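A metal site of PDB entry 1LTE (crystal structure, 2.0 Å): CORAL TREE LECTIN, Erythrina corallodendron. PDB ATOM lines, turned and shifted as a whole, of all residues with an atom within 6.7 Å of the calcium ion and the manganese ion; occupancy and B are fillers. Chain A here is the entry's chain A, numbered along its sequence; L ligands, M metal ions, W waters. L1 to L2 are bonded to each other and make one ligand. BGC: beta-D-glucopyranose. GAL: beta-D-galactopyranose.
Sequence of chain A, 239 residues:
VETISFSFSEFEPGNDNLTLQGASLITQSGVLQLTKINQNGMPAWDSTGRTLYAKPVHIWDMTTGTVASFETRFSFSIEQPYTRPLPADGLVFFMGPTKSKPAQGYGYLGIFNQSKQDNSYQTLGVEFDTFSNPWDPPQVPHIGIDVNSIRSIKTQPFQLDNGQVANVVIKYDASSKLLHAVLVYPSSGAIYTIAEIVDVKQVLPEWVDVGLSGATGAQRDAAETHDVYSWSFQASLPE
The calcium ion is bound by water W2 (2.3 Å), water W3 (2.3 Å), OD2 of Asp 136 (2.4 Å), OD1 of Asn 133 (2.4 Å), OD1 of Asp 129 (2.5 Å), OD2 of Asp 129 (2.5 Å) and O of Phe 131 (2.5 Å).
The backbone NH (N) of Glu 127 is in hydrogen-bond range of the backbone carbonyl oxygen (O) of Gly 144.
The manganese ion is bound by water W1 (2.1 Å), water W4 (2.2 Å), the side-chain carboxylate of Asp 136 (2.2 Å), the side-chain carboxylate of Glu 127 (2.2 Å), the side-chain carboxylate of Asp 129 (2.2 Å) and a ring nitrogen (NE2) of His 142 (2.4 Å).
The manganese ion has six donor atoms within binding distance.
Four residues have an atom within 4 Å of the calcium ion: Asp 129, Phe 131, Asn 133 and Asp 136.
The nearest printed residue that does not touch the calcium ion is Trp 135 (4.4 Å).
Within 4 Å of the manganese ion: Glu 127, Asp 129, Asp 136 and His 142.
The nearest printed residue that does not touch the manganese ion is Ser 152 (4.2 Å).
Water W3 lies within hydrogen-bond range of the backbone carbonyl oxygen (O) of Gly 107 (2.8 Å) and the indole nitrogen (NE1) of Trp 135 (3.1 Å).
Water W4 lies within hydrogen-bond range of OE1 of Glu 127 and O of Ile 150.
An oxygen (O3) of GAL L2 lies within hydrogen-bond range of the side-chain amide nitrogen (ND2) of Asn 133 (3.0 Å).
O3 of GAL L2 sits at hydrogen-bond distance from N of Gly 107 (2.9 Å).
An oxygen (O3) of GAL L2 is in hydrogen-bond range of the side-chain carboxylate (OD1) of Asp 89 (2.8 Å).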
ATOM      1  N   ASP A  89      -3.160 -14.432 -24.900  1.00  0.00           N
ATOM      2  CA  ASP A  89      -3.131 -15.894 -24.729  1.00  0.00           C
ATOM      3  C   ASP A  89      -4.400 -16.565 -25.205  1.00  0.00           C
ATOM      4  O   ASP A  89      -4.354 -17.731 -25.603  1.00  0.00           O
ATOM      5  CB  ASP A  89      -2.890 -16.284 -23.263  1.00  0.00           C
ATOM      6  CG  ASP A  89      -1.397 -16.396 -22.969  1.00  0.00           C
ATOM      7  OD1 ASP A  89      -0.738 -17.390 -23.308  1.00  0.00           O
ATOM      8  OD2 ASP A  89      -0.853 -15.473 -22.394  1.00  0.00           O
ATOM      9  N   TYR A 106      -2.388 -15.501 -18.209  1.00  0.00           N
ATOM     10  CA  TYR A 106      -1.509 -15.936 -19.299  1.00  0.00           C
ATOM     11  C   TYR A 106      -2.059 -17.222 -19.877  1.00  0.00           C
ATOM     12  O   TYR A 106      -3.284 -17.301 -20.029  1.00  0.00           O
ATOM     13  CB  TYR A 106      -0.042 -16.143 -18.802  1.00  0.00           C
ATOM     14  CG  TYR A 106       0.510 -15.022 -17.950  1.00  0.00           C
ATOM     15  CD1 TYR A 106       0.406 -13.710 -18.356  1.00  0.00           C
ATOM     16  CD2 TYR A 106       1.063 -15.336 -16.740  1.00  0.00           C
ATOM     17  CE1 TYR A 106       0.869 -12.695 -17.546  1.00  0.00           C
ATOM     18  CE2 TYR A 106       1.527 -14.346 -15.930  1.00  0.00           C
ATOM     19  CZ  TYR A 106       1.437 -13.033 -16.337  1.00  0.00           C
ATOM     20  OH  TYR A 106       1.918 -12.068 -15.495  1.00  0.00           O
ATOM     21  N   GLY A 107      -1.232 -18.245 -20.166  1.00  0.00           N
ATOM     22  CA  GLY A 107      -1.694 -19.516 -20.710  1.00  0.00           C
ATOM     23  C   GLY A 107      -2.698 -20.252 -19.847  1.00  0.00           C
ATOM     24  O   GLY A 107      -3.341 -21.174 -20.322  1.00  0.00           O
ATOM     25  N   TYR A 108      -2.897 -19.900 -18.583  1.00  0.00           N
ATOM     26  CA  TYR A 108      -3.884 -20.606 -17.767  1.00  0.00           C
ATOM     27  C   TYR A 108      -5.265 -20.018 -17.954  1.00  0.00           C
ATOM     28  O   TYR A 108      -6.258 -20.514 -17.382  1.00  0.00           O
ATOM     29  CB  TYR A 108      -3.491 -20.563 -16.315  1.00  0.00           C
ATOM     30  CG  TYR A 108      -2.166 -21.281 -16.120  1.00  0.00           C
ATOM     31  CD1 TYR A 108      -2.011 -22.598 -16.501  1.00  0.00           C
ATOM     32  CD2 TYR A 108      -1.106 -20.579 -15.598  1.00  0.00           C
ATOM     33  CE1 TYR A 108      -0.791 -23.209 -16.371  1.00  0.00           C
ATOM     34  CE2 TYR A 108       0.113 -21.198 -15.479  1.00  0.00           C
ATOM     35  CZ  TYR A 108       0.260 -22.503 -15.859  1.00  0.00           C
ATOM     36  OH  TYR A 108       1.500 -23.102 -15.748  1.00  0.00           O
ATOM     37  N   LEU A 109      -5.310 -18.910 -18.706  1.00  0.00           N
ATOM     38  CA  LEU A 109      -6.510 -18.186 -19.101  1.00  0.00           C
ATOM     39  C   LEU A 109      -7.469 -17.681 -18.027  1.00  0.00           C
ATOM     40  O   LEU A 109      -8.649 -17.478 -18.303  1.00  0.00           O
ATOM     41  CB  LEU A 109      -7.253 -19.094 -20.124  1.00  0.00           C
ATOM     42  CG  LEU A 109      -6.513 -19.649 -21.362  1.00  0.00           C
ATOM     43  CD1 LEU A 109      -7.419 -20.606 -22.117  1.00  0.00           C
ATOM     44  CD2 LEU A 109      -6.083 -18.522 -22.290  1.00  0.00           C
ATOM     45  N   GLU A 127     -11.857 -23.589 -24.851  1.00  0.00           N
ATOM     46  CA  GLU A 127     -10.930 -22.504 -25.148  1.00  0.00           C
ATOM     47  C   GLU A 127     -10.702 -22.210 -26.620  1.00  0.00           C
ATOM     48  O   GLU A 127     -11.003 -23.026 -27.508  1.00  0.00           O
ATOM     49  CB  GLU A 127      -9.585 -22.809 -24.499  1.00  0.00           C
ATOM     50  CG  GLU A 127      -8.984 -24.092 -25.066  1.00  0.00           C
ATOM     51  CD  GLU A 127      -7.553 -24.362 -24.661  1.00  0.00           C
ATOM     52  OE1 GLU A 127      -7.205 -24.201 -23.497  1.00  0.00           O
ATOM     53  OE2 GLU A 127      -6.749 -24.708 -25.539  1.00  0.00           O
ATOM     54  N   ASP A 129      -7.523 -20.793 -27.919  1.00  0.00           N
ATOM     55  CA  ASP A 129      -6.146 -20.577 -27.538  1.00  0.00           C
ATOM     56  C   ASP A 129      -5.252 -20.036 -28.646  1.00  0.00           C
ATOM     57  O   ASP A 129      -5.113 -20.659 -29.698  1.00  0.00           O
ATOM     58  CB  ASP A 129      -5.643 -21.936 -27.021  1.00  0.00           C
ATOM     59  CG  ASP A 129      -4.325 -21.872 -26.251  1.00  0.00           C
ATOM     60  OD1 ASP A 129      -3.568 -20.914 -26.381  1.00  0.00           O
ATOM     61  OD2 ASP A 129      -4.062 -22.796 -25.512  1.00  0.00           O
ATOM     62  N   THR A 130      -4.615 -18.904 -28.397  1.00  0.00           N
ATOM     63  CA  THR A 130      -3.793 -18.279 -29.427  1.00  0.00           C
ATOM     64  C   THR A 130      -2.293 -18.397 -29.215  1.00  0.00           C
ATOM     65  O   THR A 130      -1.558 -17.932 -30.097  1.00  0.00           O
ATOM     66  CB  THR A 130      -4.160 -16.787 -29.558  1.00  0.00           C
ATOM     67  OG1 THR A 130      -3.871 -16.184 -28.304  1.00  0.00           O
ATOM     68  CG2 THR A 130      -5.616 -16.575 -29.922  1.00  0.00           C
ATOM     69  N   PHE A 131      -1.805 -19.018 -28.134  1.00  0.00           N
ATOM     70  CA  PHE A 131      -0.369 -19.108 -27.927  1.00  0.00           C
ATOM     71  C   PHE A 131       0.001 -20.540 -27.581  1.00  0.00           C
ATOM     72  O   PHE A 131      -0.591 -21.096 -26.683  1.00  0.00           O
ATOM     73  CB  PHE A 131       0.035 -18.166 -26.807  1.00  0.00           C
ATOM     74  CG  PHE A 131       1.521 -18.241 -26.512  1.00  0.00           C
ATOM     75  CD1 PHE A 131       2.399 -17.488 -27.265  1.00  0.00           C
ATOM     76  CD2 PHE A 131       2.017 -19.081 -25.523  1.00  0.00           C
ATOM     77  CE1 PHE A 131       3.758 -17.591 -27.053  1.00  0.00           C
ATOM     78  CE2 PHE A 131       3.375 -19.175 -25.317  1.00  0.00           C
ATOM     79  CZ  PHE A 131       4.252 -18.430 -26.082  1.00  0.00           C
ATOM     80  N   SER A 132       0.981 -21.170 -28.231  1.00  0.00           N
ATOM     81  CA  SER A 132       1.341 -22.524 -27.911  1.00  0.00           C
ATOM     82  C   SER A 132       2.295 -22.660 -26.723  1.00  0.00           C
ATOM     83  O   SER A 132       3.482 -22.303 -26.763  1.00  0.00           O
ATOM     84  CB  SER A 132       1.946 -23.132 -29.163  1.00  0.00           C
ATOM     85  OG  SER A 132       2.139 -24.526 -29.067  1.00  0.00           O
ATOM     86  N   ASN A 133       1.743 -23.094 -25.594  1.00  0.00           N
ATOM     87  CA  ASN A 133       2.469 -23.318 -24.354  1.00  0.00           C
ATOM     88  C   ASN A 133       3.100 -24.720 -24.364  1.00  0.00           C
ATOM     89  O   ASN A 133       2.764 -25.492 -25.253  1.00  0.00           O
ATOM     90  CB  ASN A 133       1.527 -23.237 -23.175  1.00  0.00           C
ATOM     91  CG  ASN A 133       1.031 -21.841 -22.898  1.00  0.00           C
ATOM     92  OD1 ASN A 133      -0.023 -21.413 -23.353  1.00  0.00           O
ATOM     93  ND2 ASN A 133       1.765 -21.039 -22.179  1.00  0.00           N
ATOM     94  N   TRP A 135       2.316 -27.369 -22.922  1.00  0.00           N
ATOM     95  CA  TRP A 135       1.260 -28.353 -22.896  1.00  0.00           C
ATOM     96  C   TRP A 135       0.374 -28.298 -24.121  1.00  0.00           C
ATOM     97  O   TRP A 135      -0.485 -29.163 -24.276  1.00  0.00           O
ATOM     98  CB  TRP A 135       0.388 -28.147 -21.645  1.00  0.00           C
ATOM     99  CG  TRP A 135      -0.189 -26.740 -21.488  1.00  0.00           C
ATOM    100  CD1 TRP A 135      -1.310 -26.319 -22.164  1.00  0.00           C
ATOM    101  CD2 TRP A 135       0.344 -25.757 -20.696  1.00  0.00           C
ATOM    102  NE1 TRP A 135      -1.466 -25.075 -21.803  1.00  0.00           N
ATOM    103  CE2 TRP A 135      -0.524 -24.705 -20.919  1.00  0.00           C
ATOM    104  CE3 TRP A 135       1.420 -25.635 -19.836  1.00  0.00           C
ATOM    105  CZ2 TRP A 135      -0.325 -23.494 -20.297  1.00  0.00           C
ATOM    106  CZ3 TRP A 135       1.612 -24.421 -19.207  1.00  0.00           C
ATOM    107  CH2 TRP A 135       0.744 -23.361 -19.436  1.00  0.00           C
ATOM    108  N   ASP A 136       0.544 -27.348 -25.021  1.00  0.00           N
ATOM    109  CA  ASP A 136      -0.323 -27.245 -26.177  1.00  0.00           C
ATOM    110  C   ASP A 136       0.167 -28.014 -27.371  1.00  0.00           C
ATOM    111  O   ASP A 136       1.372 -28.239 -27.491  1.00  0.00           O
ATOM    112  CB  ASP A 136      -0.470 -25.802 -26.582  1.00  0.00           C
ATOM    113  CG  ASP A 136      -1.409 -25.028 -25.682  1.00  0.00           C
ATOM    114  OD1 ASP A 136      -2.456 -25.539 -25.326  1.00  0.00           O
ATOM    115  OD2 ASP A 136      -1.045 -23.925 -25.308  1.00  0.00           O
ATOM    116  N   PRO A 137      -0.681 -28.390 -28.326  1.00  0.00           N
ATOM    117  CA  PRO A 137      -0.260 -28.772 -29.655  1.00  0.00           C
ATOM    118  C   PRO A 137       0.482 -27.613 -30.313  1.00  0.00           C
ATOM    119  O   PRO A 137       0.234 -26.463 -29.958  1.00  0.00           O
ATOM    120  CB  PRO A 137      -1.535 -29.135 -30.355  1.00  0.00           C
ATOM    121  CG  PRO A 137      -2.543 -28.253 -29.685  1.00  0.00           C
ATOM    122  CD  PRO A 137      -2.133 -28.382 -28.220  1.00  0.00           C
ATOM    123  N   VAL A 140      -1.515 -23.092 -33.460  1.00  0.00           N
ATOM    124  CA  VAL A 140      -2.347 -22.099 -32.801  1.00  0.00           C
ATOM    125  C   VAL A 140      -2.846 -21.171 -33.908  1.00  0.00           C
ATOM    126  O   VAL A 140      -2.125 -21.025 -34.907  1.00  0.00           O
ATOM    127  CB  VAL A 140      -1.599 -21.240 -31.728  1.00  0.00           C
ATOM    128  CG1 VAL A 140      -1.453 -22.111 -30.503  1.00  0.00           C
ATOM    129  CG2 VAL A 140      -0.277 -20.709 -32.186  1.00  0.00           C
ATOM    130  N   HIS A 142      -6.217 -22.611 -31.655  1.00  0.00           N
ATOM    131  CA  HIS A 142      -6.934 -23.888 -31.663  1.00  0.00           C
ATOM    132  C   HIS A 142      -8.066 -23.791 -30.643  1.00  0.00           C
ATOM    133  O   HIS A 142      -8.060 -22.968 -29.719  1.00  0.00           O
ATOM    134  CB  HIS A 142      -6.032 -25.119 -31.297  1.00  0.00           C
ATOM    135  CG  HIS A 142      -5.199 -25.037 -30.023  1.00  0.00           C
ATOM    136  ND1 HIS A 142      -3.938 -24.663 -29.919  1.00  0.00           N
ATOM    137  CD2 HIS A 142      -5.657 -25.343 -28.766  1.00  0.00           C
ATOM    138  CE1 HIS A 142      -3.587 -24.713 -28.657  1.00  0.00           C
ATOM    139  NE2 HIS A 142      -4.631 -25.122 -27.986  1.00  0.00           N
ATOM    140  N   ILE A 143      -9.101 -24.534 -30.960  1.00  0.00           N
ATOM    141  CA  ILE A 143     -10.243 -24.654 -30.083  1.00  0.00           C
ATOM    142  C   ILE A 143      -9.839 -25.851 -29.206  1.00  0.00           C
ATOM    143  O   ILE A 143      -9.288 -26.828 -29.743  1.00  0.00           O
ATOM    144  CB  ILE A 143     -11.543 -25.045 -30.839  1.00  0.00           C
ATOM    145  CG1 ILE A 143     -11.772 -24.110 -32.032  1.00  0.00           C
ATOM    146  CG2 ILE A 143     -12.735 -24.955 -29.860  1.00  0.00           C
ATOM    147  CD1 ILE A 143     -12.883 -24.564 -32.991  1.00  0.00           C
ATOM    148  N   GLY A 144     -10.090 -25.867 -27.911  1.00  0.00           N
ATOM    149  CA  GLY A 144      -9.741 -27.034 -27.093  1.00  0.00           C
ATOM    150  C   GLY A 144     -10.841 -27.304 -26.066  1.00  0.00           C
ATOM    151  O   GLY A 144     -11.577 -26.372 -25.706  1.00  0.00           O
ATOM    152  N   ASP A 146     -11.382 -28.447 -22.377  1.00  0.00           N
ATOM    153  CA  ASP A 146     -10.648 -28.561 -21.118  1.00  0.00           C
ATOM    154  C   ASP A 146     -11.500 -29.143 -20.021  1.00  0.00           C
ATOM    155  O   ASP A 146     -12.561 -28.588 -19.673  1.00  0.00           O
ATOM    156  CB  ASP A 146     -10.160 -27.194 -20.684  1.00  0.00           C
ATOM    157  CG  ASP A 146      -9.319 -26.483 -21.731  1.00  0.00           C
ATOM    158  OD1 ASP A 146      -8.962 -27.106 -22.714  1.00  0.00           O
ATOM    159  OD2 ASP A 146      -9.041 -25.302 -21.539  1.00  0.00           O
ATOM    160  N   ILE A 150      -5.781 -27.412 -18.122  1.00  0.00           N
ATOM    161  CA  ILE A 150      -5.531 -26.537 -19.268  1.00  0.00           C
ATOM    162  C   ILE A 150      -4.995 -27.446 -20.423  1.00  0.00           C
ATOM    163  O   ILE A 150      -4.862 -27.082 -21.566  1.00  0.00           O
ATOM    164  CB  ILE A 150      -4.507 -25.434 -18.808  1.00  0.00           C
ATOM    165  CG1 ILE A 150      -4.443 -24.346 -19.870  1.00  0.00           C
ATOM    166  CG2 ILE A 150      -3.134 -25.999 -18.533  1.00  0.00           C
ATOM    167  CD1 ILE A 150      -5.783 -23.570 -20.068  1.00  0.00           C
ATOM    168  N   ARG A 151      -4.695 -28.709 -20.142  1.00  0.00           N
ATOM    169  CA  ARG A 151      -4.179 -29.668 -21.116  1.00  0.00           C
ATOM    170  C   ARG A 151      -5.433 -30.253 -21.754  1.00  0.00           C
ATOM    171  O   ARG A 151      -5.966 -31.224 -21.213  1.00  0.00           O
ATOM    172  CB  ARG A 151      -3.341 -30.532 -20.197  1.00  0.00           C
ATOM    173  CG  ARG A 151      -2.516 -31.681 -20.691  1.00  0.00           C
ATOM    174  CD  ARG A 151      -1.226 -31.754 -19.835  1.00  0.00           C
ATOM    175  NE  ARG A 151      -1.365 -31.791 -18.382  1.00  0.00           N
ATOM    176  CZ  ARG A 151      -1.504 -32.892 -17.639  1.00  0.00           C
ATOM    177  NH1 ARG A 151      -1.618 -34.109 -18.169  1.00  0.00           N
ATOM    178  NH2 ARG A 151      -1.583 -32.770 -16.314  1.00  0.00           N
ATOM    179  N   SER A 152      -5.971 -29.701 -22.844  1.00  0.00           N
ATOM    180  CA  SER A 152      -7.197 -30.180 -23.487  1.00  0.00           C
ATOM    181  C   SER A 152      -7.278 -31.647 -23.800  1.00  0.00           C
ATOM    182  O   SER A 152      -6.283 -32.271 -24.174  1.00  0.00           O
ATOM    183  CB  SER A 152      -7.472 -29.425 -24.820  1.00  0.00           C
ATOM    184  OG  SER A 152      -7.087 -28.108 -24.523  1.00  0.00           O
ATOM    185  N   THR A 155      -8.433 -31.107 -29.303  1.00  0.00           N
ATOM    186  CA  THR A 155      -8.014 -29.845 -29.902  1.00  0.00           C
ATOM    187  C   THR A 155      -8.423 -29.757 -31.374  1.00  0.00           C
ATOM    188  O   THR A 155      -8.533 -30.807 -32.016  1.00  0.00           O
ATOM    189  CB  THR A 155      -6.500 -29.879 -29.602  1.00  0.00           C
ATOM    190  OG1 THR A 155      -6.322 -28.844 -28.647  1.00  0.00           O
ATOM    191  CG2 THR A 155      -5.611 -29.801 -30.808  1.00  0.00           C
HETATM  192  C2  BGC L   1       9.034 -14.932 -20.629  1.00  0.00           C
HETATM  193  C3  BGC L   1       7.517 -15.052 -20.619  1.00  0.00           C
HETATM  194  C4  BGC L   1       7.181 -16.584 -20.502  1.00  0.00           C
HETATM  195  C5  BGC L   1       7.878 -17.257 -19.283  1.00  0.00           C
HETATM  196  C6  BGC L   1       7.864 -18.820 -19.314  1.00  0.00           C
HETATM  197  C1  BGC L   1       9.637 -15.533 -19.348  1.00  0.00           C
HETATM  198  O1  BGC L   1      11.051 -15.469 -19.396  1.00  0.00           O
HETATM  199  O2  BGC L   1       9.366 -13.562 -20.807  1.00  0.00           O
HETATM  200  O3  BGC L   1       7.027 -14.449 -21.817  1.00  0.00           O
HETATM  201  O4  BGC L   1       5.759 -16.762 -20.282  1.00  0.00           O
HETATM  202  O5  BGC L   1       9.272 -16.902 -19.218  1.00  0.00           O
HETATM  203  O6  BGC L   1       7.196 -19.383 -20.421  1.00  0.00           O
HETATM  204  C1  GAL L   2       4.919 -17.056 -21.403  1.00  0.00           C
HETATM  205  C2  GAL L   2       3.531 -17.467 -20.867  1.00  0.00           C
HETATM  206  C3  GAL L   2       2.559 -17.711 -22.028  1.00  0.00           C
HETATM  207  C4  GAL L   2       2.486 -16.409 -22.848  1.00  0.00           C
HETATM  208  C5  GAL L   2       3.884 -15.995 -23.345  1.00  0.00           C
HETATM  209  C6  GAL L   2       3.887 -14.654 -24.094  1.00  0.00           C
HETATM  210  O2  GAL L   2       3.553 -18.626 -20.062  1.00  0.00           O
HETATM  211  O3  GAL L   2       1.268 -18.104 -21.528  1.00  0.00           O
HETATM  212  O4  GAL L   2       1.950 -15.378 -22.032  1.00  0.00           O
HETATM  213  O5  GAL L   2       4.788 -15.884 -22.233  1.00  0.00           O
HETATM  214  O6  GAL L   2       5.215 -14.385 -24.496  1.00  0.00           O
HETATM  215 CA    CA M   1      -1.963 -21.786 -24.747  1.00  0.00          CA
HETATM  216 MN    MN M   2      -4.553 -24.976 -25.595  1.00  0.00          MN
HETATM  217  O   HOH W   1      -4.825 -27.100 -25.614  1.00  0.00           O
HETATM  218  O   HOH W   2      -2.262 -19.568 -24.159  1.00  0.00           O
HETATM  219  O   HOH W   3      -2.992 -22.516 -22.776  1.00  0.00           O
HETATM  220  O   HOH W   4      -4.632 -24.990 -23.411  1.00  0.00           O
